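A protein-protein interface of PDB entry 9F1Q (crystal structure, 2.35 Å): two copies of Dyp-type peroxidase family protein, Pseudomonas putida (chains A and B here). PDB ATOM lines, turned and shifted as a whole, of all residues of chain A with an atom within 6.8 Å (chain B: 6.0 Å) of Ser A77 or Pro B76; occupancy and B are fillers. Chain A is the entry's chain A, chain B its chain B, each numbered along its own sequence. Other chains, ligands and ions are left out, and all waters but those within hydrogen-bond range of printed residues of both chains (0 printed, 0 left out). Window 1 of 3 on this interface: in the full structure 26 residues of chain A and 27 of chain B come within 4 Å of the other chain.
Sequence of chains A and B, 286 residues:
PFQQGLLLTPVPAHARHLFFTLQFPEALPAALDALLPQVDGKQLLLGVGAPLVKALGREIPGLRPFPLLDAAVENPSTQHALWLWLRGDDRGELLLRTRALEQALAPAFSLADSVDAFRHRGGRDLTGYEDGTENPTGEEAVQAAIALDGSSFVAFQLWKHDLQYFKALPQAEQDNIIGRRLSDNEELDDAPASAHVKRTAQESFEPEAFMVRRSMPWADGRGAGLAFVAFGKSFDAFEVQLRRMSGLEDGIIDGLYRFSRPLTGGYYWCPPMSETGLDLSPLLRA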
ATOM      1  N   PRO A  65      21.666  -4.468   8.342  1.00  0.00           N
ATOM      2  CA  PRO A  65      21.328  -3.510   9.403  1.00  0.00           C
ATOM      3  C   PRO A  65      22.268  -2.312   9.404  1.00  0.00           C
ATOM      4  O   PRO A  65      23.351  -2.330   8.813  1.00  0.00           O
ATOM      5  CB  PRO A  65      21.467  -4.329  10.691  1.00  0.00           C
ATOM      6  CG  PRO A  65      22.325  -5.485  10.330  1.00  0.00           C
ATOM      7  CD  PRO A  65      22.060  -5.779   8.888  1.00  0.00           C
ATOM      8  N   PHE A  66      21.821  -1.254  10.075  1.00  0.00           N
ATOM      9  CA  PHE A  66      22.629  -0.049  10.211  1.00  0.00           C
ATOM     10  C   PHE A  66      23.972  -0.407  10.843  1.00  0.00           C
ATOM     11  O   PHE A  66      24.005  -1.140  11.841  1.00  0.00           O
ATOM     12  CB  PHE A  66      21.888   0.987  11.061  1.00  0.00           C
ATOM     13  CG  PHE A  66      22.533   2.349  11.075  1.00  0.00           C
ATOM     14  CD1 PHE A  66      23.535   2.651  11.986  1.00  0.00           C
ATOM     15  CD2 PHE A  66      22.123   3.332  10.188  1.00  0.00           C
ATOM     16  CE1 PHE A  66      24.124   3.906  12.003  1.00  0.00           C
ATOM     17  CE2 PHE A  66      22.706   4.589  10.202  1.00  0.00           C
ATOM     18  CZ  PHE A  66      23.709   4.874  11.111  1.00  0.00           C
ATOM     19  N   PRO A  67      25.088   0.080  10.303  1.00  0.00           N
ATOM     20  CA  PRO A  67      26.398  -0.432  10.722  1.00  0.00           C
ATOM     21  C   PRO A  67      26.773   0.023  12.125  1.00  0.00           C
ATOM     22  O   PRO A  67      26.152   0.902  12.727  1.00  0.00           O
ATOM     23  CB  PRO A  67      27.351   0.146   9.673  1.00  0.00           C
ATOM     24  CG  PRO A  67      26.692   1.411   9.243  1.00  0.00           C
ATOM     25  CD  PRO A  67      25.212   1.121   9.267  1.00  0.00           C
ATOM     26  N   LEU A  68      27.822  -0.609  12.644  1.00  0.00           N
ATOM     27  CA  LEU A  68      28.385  -0.299  13.953  1.00  0.00           C
ATOM     28  C   LEU A  68      29.732   0.375  13.729  1.00  0.00           C
ATOM     29  O   LEU A  68      30.694  -0.276  13.309  1.00  0.00           O
ATOM     30  CB  LEU A  68      28.538  -1.563  14.795  1.00  0.00           C
ATOM     31  CG  LEU A  68      29.160  -1.391  16.183  1.00  0.00           C
ATOM     32  CD1 LEU A  68      28.217  -0.645  17.121  1.00  0.00           C
ATOM     33  CD2 LEU A  68      29.575  -2.734  16.768  1.00  0.00           C
ATOM     34  N   ASN A  75      27.184   7.084  16.738  1.00  0.00           N
ATOM     35  CA  ASN A  75      26.202   6.836  15.683  1.00  0.00           C
ATOM     36  C   ASN A  75      25.496   5.544  16.069  1.00  0.00           C
ATOM     37  O   ASN A  75      25.924   4.450  15.675  1.00  0.00           O
ATOM     38  CB  ASN A  75      26.852   6.716  14.305  1.00  0.00           C
ATOM     39  CG  ASN A  75      27.588   7.972  13.889  1.00  0.00           C
ATOM     40  OD1 ASN A  75      26.975   8.963  13.491  1.00  0.00           O
ATOM     41  ND2 ASN A  75      28.912   7.926  13.948  1.00  0.00           N
ATOM     42  N   PRO A  76      24.416   5.627  16.843  1.00  0.00           N
ATOM     43  CA  PRO A  76      23.758   4.404  17.314  1.00  0.00           C
ATOM     44  C   PRO A  76      23.074   3.652  16.183  1.00  0.00           C
ATOM     45  O   PRO A  76      22.664   4.230  15.173  1.00  0.00           O
ATOM     46  CB  PRO A  76      22.740   4.909  18.343  1.00  0.00           C
ATOM     47  CG  PRO A  76      22.611   6.375  18.127  1.00  0.00           C
ATOM     48  CD  PRO A  76      23.648   6.844  17.154  1.00  0.00           C
ATOM     49  N   SER A  77      22.966   2.339  16.366  1.00  0.00           N
ATOM     50  CA  SER A  77      22.260   1.461  15.440  1.00  0.00           C
ATOM     51  C   SER A  77      20.977   0.995  16.117  1.00  0.00           C
ATOM     52  O   SER A  77      21.019   0.199  17.061  1.00  0.00           O
ATOM     53  CB  SER A  77      23.136   0.278  15.037  1.00  0.00           C
ATOM     54  OG  SER A  77      22.448  -0.590  14.153  1.00  0.00           O
ATOM     55  N   THR A  78      19.838   1.494  15.632  1.00  0.00           N
ATOM     56  CA  THR A  78      18.526   1.173  16.189  1.00  0.00           C
ATOM     57  C   THR A  78      17.635   0.680  15.046  1.00  0.00           C
ATOM     58  O   THR A  78      16.643   1.315  14.681  1.00  0.00           O
ATOM     59  CB  THR A  78      17.918   2.382  16.905  1.00  0.00           C
ATOM     60  OG1 THR A  78      17.753   3.460  15.976  1.00  0.00           O
ATOM     61  CG2 THR A  78      18.816   2.835  18.047  1.00  0.00           C
ATOM     62  N   GLN A  79      18.006  -0.470  14.486  1.00  0.00           N
ATOM     63  CA  GLN A  79      17.335  -1.003  13.310  1.00  0.00           C
ATOM     64  C   GLN A  79      15.966  -1.566  13.679  1.00  0.00           C
ATOM     65  O   GLN A  79      15.831  -2.310  14.656  1.00  0.00           O
ATOM     66  CB  GLN A  79      18.194  -2.086  12.665  1.00  0.00           C
ATOM     67  CG  GLN A  79      17.699  -2.541  11.304  1.00  0.00           C
ATOM     68  CD  GLN A  79      17.706  -1.420  10.284  1.00  0.00           C
ATOM     69  OE1 GLN A  79      18.741  -0.801  10.031  1.00  0.00           O
ATOM     70  NE2 GLN A  79      16.548  -1.149   9.694  1.00  0.00           N
ATOM     71  N   HIS A  80      14.953  -1.213  12.895  1.00  0.00           N
ATOM     72  CA  HIS A  80      13.606  -1.736  13.063  1.00  0.00           C
ATOM     73  C   HIS A  80      13.197  -2.519  11.820  1.00  0.00           C
ATOM     74  O   HIS A  80      13.916  -2.566  10.817  1.00  0.00           O
ATOM     75  CB  HIS A  80      12.610  -0.606  13.353  1.00  0.00           C
ATOM     76  CG  HIS A  80      12.926   0.167  14.596  1.00  0.00           C
ATOM     77  ND1 HIS A  80      12.882  -0.395  15.854  1.00  0.00           N
ATOM     78  CD2 HIS A  80      13.299   1.457  14.773  1.00  0.00           C
ATOM     79  CE1 HIS A  80      13.212   0.516  16.752  1.00  0.00           C
ATOM     80  NE2 HIS A  80      13.469   1.649  16.123  1.00  0.00           N
ATOM     81  N   LEU A 263      20.370  10.314  17.377  1.00  0.00           N
ATOM     82  CA  LEU A 263      19.758   9.490  18.408  1.00  0.00           C
ATOM     83  C   LEU A 263      19.386   8.104  17.907  1.00  0.00           C
ATOM     84  O   LEU A 263      19.269   7.177  18.715  1.00  0.00           O
ATOM     85  CB  LEU A 263      18.499  10.170  18.956  1.00  0.00           C
ATOM     86  CG  LEU A 263      18.626  11.576  19.543  1.00  0.00           C
ATOM     87  CD1 LEU A 263      17.254  12.098  19.955  1.00  0.00           C
ATOM     88  CD2 LEU A 263      19.594  11.601  20.715  1.00  0.00           C
ATOM     89  N   THR A 264      19.197   7.943  16.598  1.00  0.00           N
ATOM     90  CA  THR A 264      18.777   6.678  16.013  1.00  0.00           C
ATOM     91  C   THR A 264      19.573   6.430  14.741  1.00  0.00           C
ATOM     92  O   THR A 264      20.247   7.320  14.216  1.00  0.00           O
ATOM     93  CB  THR A 264      17.273   6.662  15.691  1.00  0.00           C
ATOM     94  OG1 THR A 264      16.987   7.645  14.689  1.00  0.00           O
ATOM     95  CG2 THR A 264      16.439   6.951  16.935  1.00  0.00           C
ATOM     96  N   GLY A 265      19.490   5.198  14.249  1.00  0.00           N
ATOM     97  CA  GLY A 265      20.109   4.828  12.989  1.00  0.00           C
ATOM     98  C   GLY A 265      19.451   3.610  12.376  1.00  0.00           C
ATOM     99  O   GLY A 265      19.295   2.582  13.043  1.00  0.00           O
ATOM    100  N   GLY A 266      19.059   3.706  11.107  1.00  0.00           N
ATOM    101  CA  GLY A 266      18.412   2.588  10.450  1.00  0.00           C
ATOM    102  C   GLY A 266      18.657   2.486   8.959  1.00  0.00           C
ATOM    103  O   GLY A 266      18.752   3.500   8.260  1.00  0.00           O
ATOM    104  N   PHE B  66      28.976  -2.020  22.025  1.00  0.00           N
ATOM    105  CA  PHE B  66      27.933  -3.035  22.051  1.00  0.00           C
ATOM    106  C   PHE B  66      27.749  -3.617  20.651  1.00  0.00           C
ATOM    107  O   PHE B  66      27.694  -2.857  19.672  1.00  0.00           O
ATOM    108  CB  PHE B  66      26.624  -2.434  22.563  1.00  0.00           C
ATOM    109  CG  PHE B  66      25.551  -3.452  22.840  1.00  0.00           C
ATOM    110  CD1 PHE B  66      24.694  -3.874  21.835  1.00  0.00           C
ATOM    111  CD2 PHE B  66      25.398  -3.983  24.110  1.00  0.00           C
ATOM    112  CE1 PHE B  66      23.710  -4.811  22.091  1.00  0.00           C
ATOM    113  CE2 PHE B  66      24.415  -4.917  24.372  1.00  0.00           C
ATOM    114  CZ  PHE B  66      23.570  -5.332  23.362  1.00  0.00           C
ATOM    115  N   PRO B  67      27.658  -4.938  20.512  1.00  0.00           N
ATOM    116  CA  PRO B  67      27.726  -5.557  19.183  1.00  0.00           C
ATOM    117  C   PRO B  67      26.473  -5.300  18.360  1.00  0.00           C
ATOM    118  O   PRO B  67      25.445  -4.818  18.842  1.00  0.00           O
ATOM    119  CB  PRO B  67      27.885  -7.045  19.503  1.00  0.00           C
ATOM    120  CG  PRO B  67      27.201  -7.207  20.817  1.00  0.00           C
ATOM    121  CD  PRO B  67      27.489  -5.940  21.578  1.00  0.00           C
ATOM    122  N   LEU B  68      26.587  -5.632  17.076  1.00  0.00           N
ATOM    123  CA  LEU B  68      25.503  -5.521  16.105  1.00  0.00           C
ATOM    124  C   LEU B  68      25.064  -6.930  15.728  1.00  0.00           C
ATOM    125  O   LEU B  68      25.802  -7.654  15.050  1.00  0.00           O
ATOM    126  CB  LEU B  68      25.960  -4.740  14.875  1.00  0.00           C
ATOM    127  CG  LEU B  68      24.953  -4.559  13.739  1.00  0.00           C
ATOM    128  CD1 LEU B  68      23.838  -3.617  14.165  1.00  0.00           C
ATOM    129  CD2 LEU B  68      25.639  -4.062  12.472  1.00  0.00           C
ATOM    130  N   GLU B  74      15.244  -7.424  17.702  1.00  0.00           N
ATOM    131  CA  GLU B  74      15.959  -6.157  17.770  1.00  0.00           C
ATOM    132  C   GLU B  74      16.758  -6.073  19.066  1.00  0.00           C
ATOM    133  O   GLU B  74      16.191  -6.172  20.159  1.00  0.00           O
ATOM    134  CB  GLU B  74      14.987  -4.983  17.659  1.00  0.00           C
ATOM    135  CG  GLU B  74      14.278  -4.901  16.312  1.00  0.00           C
ATOM    136  CD  GLU B  74      13.208  -3.827  16.273  1.00  0.00           C
ATOM    137  OE1 GLU B  74      13.252  -2.914  17.121  1.00  0.00           O
ATOM    138  OE2 GLU B  74      12.327  -3.896  15.389  1.00  0.00           O
ATOM    139  N   ASN B  75      18.074  -5.896  18.935  1.00  0.00           N
ATOM    140  CA  ASN B  75      18.965  -5.570  20.049  1.00  0.00           C
ATOM    141  C   ASN B  75      19.747  -4.333  19.631  1.00  0.00           C
ATOM    142  O   ASN B  75      20.818  -4.442  19.017  1.00  0.00           O
ATOM    143  CB  ASN B  75      19.913  -6.719  20.393  1.00  0.00           C
ATOM    144  CG  ASN B  75      19.185  -7.971  20.833  1.00  0.00           C
ATOM    145  OD1 ASN B  75      18.701  -8.059  21.962  1.00  0.00           O
ATOM    146  ND2 ASN B  75      19.135  -8.964  19.955  1.00  0.00           N
ATOM    147  N   PRO B  76      19.240  -3.139  19.931  1.00  0.00           N
ATOM    148  CA  PRO B  76      19.919  -1.925  19.467  1.00  0.00           C
ATOM    149  C   PRO B  76      21.254  -1.726  20.165  1.00  0.00           C
ATOM    150  O   PRO B  76      21.459  -2.143  21.309  1.00  0.00           O
ATOM    151  CB  PRO B  76      18.935  -0.800  19.814  1.00  0.00           C
ATOM    152  CG  PRO B  76      17.952  -1.377  20.776  1.00  0.00           C
ATOM    153  CD  PRO B  76      18.153  -2.858  20.884  1.00  0.00           C
ATOM    154  N   SER B  77      22.173  -1.083  19.450  1.00  0.00           N
ATOM    155  CA  SER B  77      23.478  -0.705  19.977  1.00  0.00           C
ATOM    156  C   SER B  77      23.493   0.810  20.125  1.00  0.00           C
ATOM    157  O   SER B  77      23.510   1.536  19.125  1.00  0.00           O
ATOM    158  CB  SER B  77      24.601  -1.190  19.063  1.00  0.00           C
ATOM    159  OG  SER B  77      25.871  -0.810  19.564  1.00  0.00           O
ATOM    160  N   THR B  78      23.479   1.287  21.371  1.00  0.00           N
ATOM    161  CA  THR B  78      23.444   2.716  21.680  1.00  0.00           C
ATOM    162  C   THR B  78      24.597   3.027  22.639  1.00  0.00           C
ATOM    163  O   THR B  78      24.391   3.381  23.802  1.00  0.00           O
ATOM    164  CB  THR B  78      22.093   3.124  22.270  1.00  0.00           C
ATOM    165  OG1 THR B  78      21.868   2.406  23.489  1.00  0.00           O
ATOM    166  CG2 THR B  78      20.965   2.816  21.292  1.00  0.00           C
ATOM    167  N   GLN B 157      21.290  -3.376  29.057  1.00  0.00           N
ATOM    168  CA  GLN B 157      20.152  -3.254  28.157  1.00  0.00           C
ATOM    169  C   GLN B 157      18.936  -2.824  28.960  1.00  0.00           C
ATOM    170  O   GLN B 157      18.691  -3.343  30.052  1.00  0.00           O
ATOM    171  CB  GLN B 157      19.829  -4.571  27.440  1.00  0.00           C
ATOM    172  CG  GLN B 157      20.830  -5.006  26.389  1.00  0.00           C
ATOM    173  CD  GLN B 157      20.452  -6.338  25.770  1.00  0.00           C
ATOM    174  OE1 GLN B 157      20.284  -7.335  26.473  1.00  0.00           O
ATOM    175  NE2 GLN B 157      20.304  -6.360  24.451  1.00  0.00           N
ATOM    176  N   PRO B 262      14.647  -5.005  24.151  1.00  0.00           N
ATOM    177  CA  PRO B 262      15.596  -4.016  24.683  1.00  0.00           C
ATOM    178  C   PRO B 262      15.520  -2.703  23.913  1.00  0.00           C
ATOM    179  O   PRO B 262      15.474  -2.688  22.681  1.00  0.00           O
ATOM    180  CB  PRO B 262      16.958  -4.695  24.493  1.00  0.00           C
ATOM    181  CG  PRO B 262      16.750  -5.611  23.323  1.00  0.00           C
ATOM    182  CD  PRO B 262      15.321  -6.082  23.404  1.00  0.00           C
ATOM    183  N   LEU B 263      15.506  -1.596  24.657  1.00  0.00           N
ATOM    184  CA  LEU B 263      15.503  -0.266  24.062  1.00  0.00           C
ATOM    185  C   LEU B 263      16.901   0.309  23.888  1.00  0.00           C
ATOM    186  O   LEU B 263      17.091   1.192  23.043  1.00  0.00           O
ATOM    187  CB  LEU B 263      14.672   0.700  24.916  1.00  0.00           C
ATOM    188  CG  LEU B 263      13.212   0.328  25.180  1.00  0.00           C
ATOM    189  CD1 LEU B 263      12.558   1.349  26.100  1.00  0.00           C
ATOM    190  CD2 LEU B 263      12.429   0.192  23.880  1.00  0.00           C
ATOM    191  N   THR B 264      17.878  -0.161  24.663  1.00  0.00           N
ATOM    192  CA  THR B 264      19.242   0.348  24.609  1.00  0.00           C
ATOM    193  C   THR B 264      20.214  -0.822  24.687  1.00  0.00           C
ATOM    194  O   THR B 264      19.841  -1.953  25.011  1.00  0.00           O
ATOM    195  CB  THR B 264      19.541   1.337  25.750  1.00  0.00           C
ATOM    196  OG1 THR B 264      19.465   0.655  27.008  1.00  0.00           O
ATOM    197  CG2 THR B 264      18.556   2.501  25.748  1.00  0.00           C
ATOM    198  N   GLY B 265      21.475  -0.536  24.375  1.00  0.00           N
ATOM    199  CA  GLY B 265      22.539  -1.514  24.498  1.00  0.00           C
ATOM    200  C   GLY B 265      23.902  -0.865  24.628  1.00  0.00           C
ATOM    201  O   GLY B 265      24.277  -0.024  23.804  1.00  0.00           O
ATOM    202  N   GLY B 266      24.653  -1.248  25.659  1.00  0.00           N
ATOM    203  CA  GLY B 266      25.967  -0.677  25.877  1.00  0.00           C
ATOM    204  C   GLY B 266      26.970  -1.597  26.542  1.00  0.00           C
ATOM    205  O   GLY B 266      26.617  -2.393  27.418  1.00  0.00           O
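The backbone carbonyl oxygen of Phe A66 lies within hydrogen-bond range of the side-chain hydroxyl of Ser A77 (2.8 Å).
N of Phe A66 is in hydrogen-bond range of OE1 of Gln A79.
The backbone NH (N) of Gly A265 lies close to the backbone carbonyl oxygen (O) of Pro A76 (3.4 Å).
The backbone NH of Thr A78 is in hydrogen-bond range of the backbone carbonyl oxygen of Gly A265, 2.9 Å away.
The backbone carbonyl oxygen (O) of Phe B66 lies within hydrogen-bond range of the side-chain hydroxyl (OG) of Ser B77 (2.7 Å).
The backbone carbonyl oxygen (O) of Pro B76 sits close to the backbone NH (N) of Gly B265 (3.5 Å).
Phe A66 touches Leu B68, and with the chains exchanged Leu A68 touches Phe B66.
Leu A68 touches Ser B77, and with the chains exchanged Ser A77 touches Leu B68.
Pro A76 touches Ser B77, and with the chains exchanged Ser A77 touches Pro B76.
Ser B77 touches its own counterpart, Ser A77.
Positions printed for both chains: 66, 67, 68, 75, 76, 77, 78, 263, 264, 265 and 266.
Of chain B, only Leu B68 (3.3 Å), Pro B76 (3.4 Å) and Ser B77 (2.9 Å) come within 4 Å of Ser A77.
Of chain A, only Ser A77 (3.4 Å) comes within 4 Å of Pro B76.
Printed residues of chain A within 4 Å of Glu B74: Gln A79 (3.4 Å) and His A80 (2.8 Å).
Of the printed residues of chain A, Thr B78 touches Thr A78.
Of the printed residues of chain A, Ser B77 touches Leu A68, Pro A76 and Ser A77.
Of the printed residues of chain B, His A80 touches Glu B74 (2.8 Å).
The nearest residue of chain B that does not touch Ser A77 is Thr B78 (5.0 Å).
The nearest residue of chain A that does not touch Pro B76 is Thr A78 (4.04 Å).
The nearest printed residue of chain A that does not touch Ser B77 is Thr A78 (5.0 Å).
Printed residues of chain B that touch a printed residue of chain A: Phe B66, Leu B68, Glu B74, Pro B76, Ser B77 and Thr B78.
Of the 14 printed residues of chain A, 7 touch a printed residue of chain B.
Printed residues of chain A that touch a printed residue of chain B: Phe A66, Leu A68, Pro A76, Ser A77, Thr A78, Gln A79 and His A80.
Hydrophobic or aromatic side chains of chain A within 4 Å of the printed part of chain B: Leu A68, Pro A76 and His A80.
Among the printed residues, 10 pairs touch across the chains.
O of Phe A66 touches CD1 of Leu B68, at 3.4 Å.
CD1 of Leu A68 touches O of Phe B66 (3.4 Å).
CD1 of Leu A68 touches OG of Ser B77 (3.4 Å).
Ser B77 touches Pro A76.
OG of Ser A77 touches CD1 of Leu B68, 3.3 Å away.
Ser A77 touches Pro B76 (O to CA, 3.4 Å).
CG2 of Thr B78 touches CG2 of Thr A78, 3.9 Å away.
O of Gln A79 touches CD of Glu B74, 3.4 Å away.
N of Ser A77 sits at hydrogen-bond distance from O of Ser B77 (2.9 Å).
ND1 of His A80 sits at hydrogen-bond distance from OE1 of Glu B74, 2.8 Å away.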
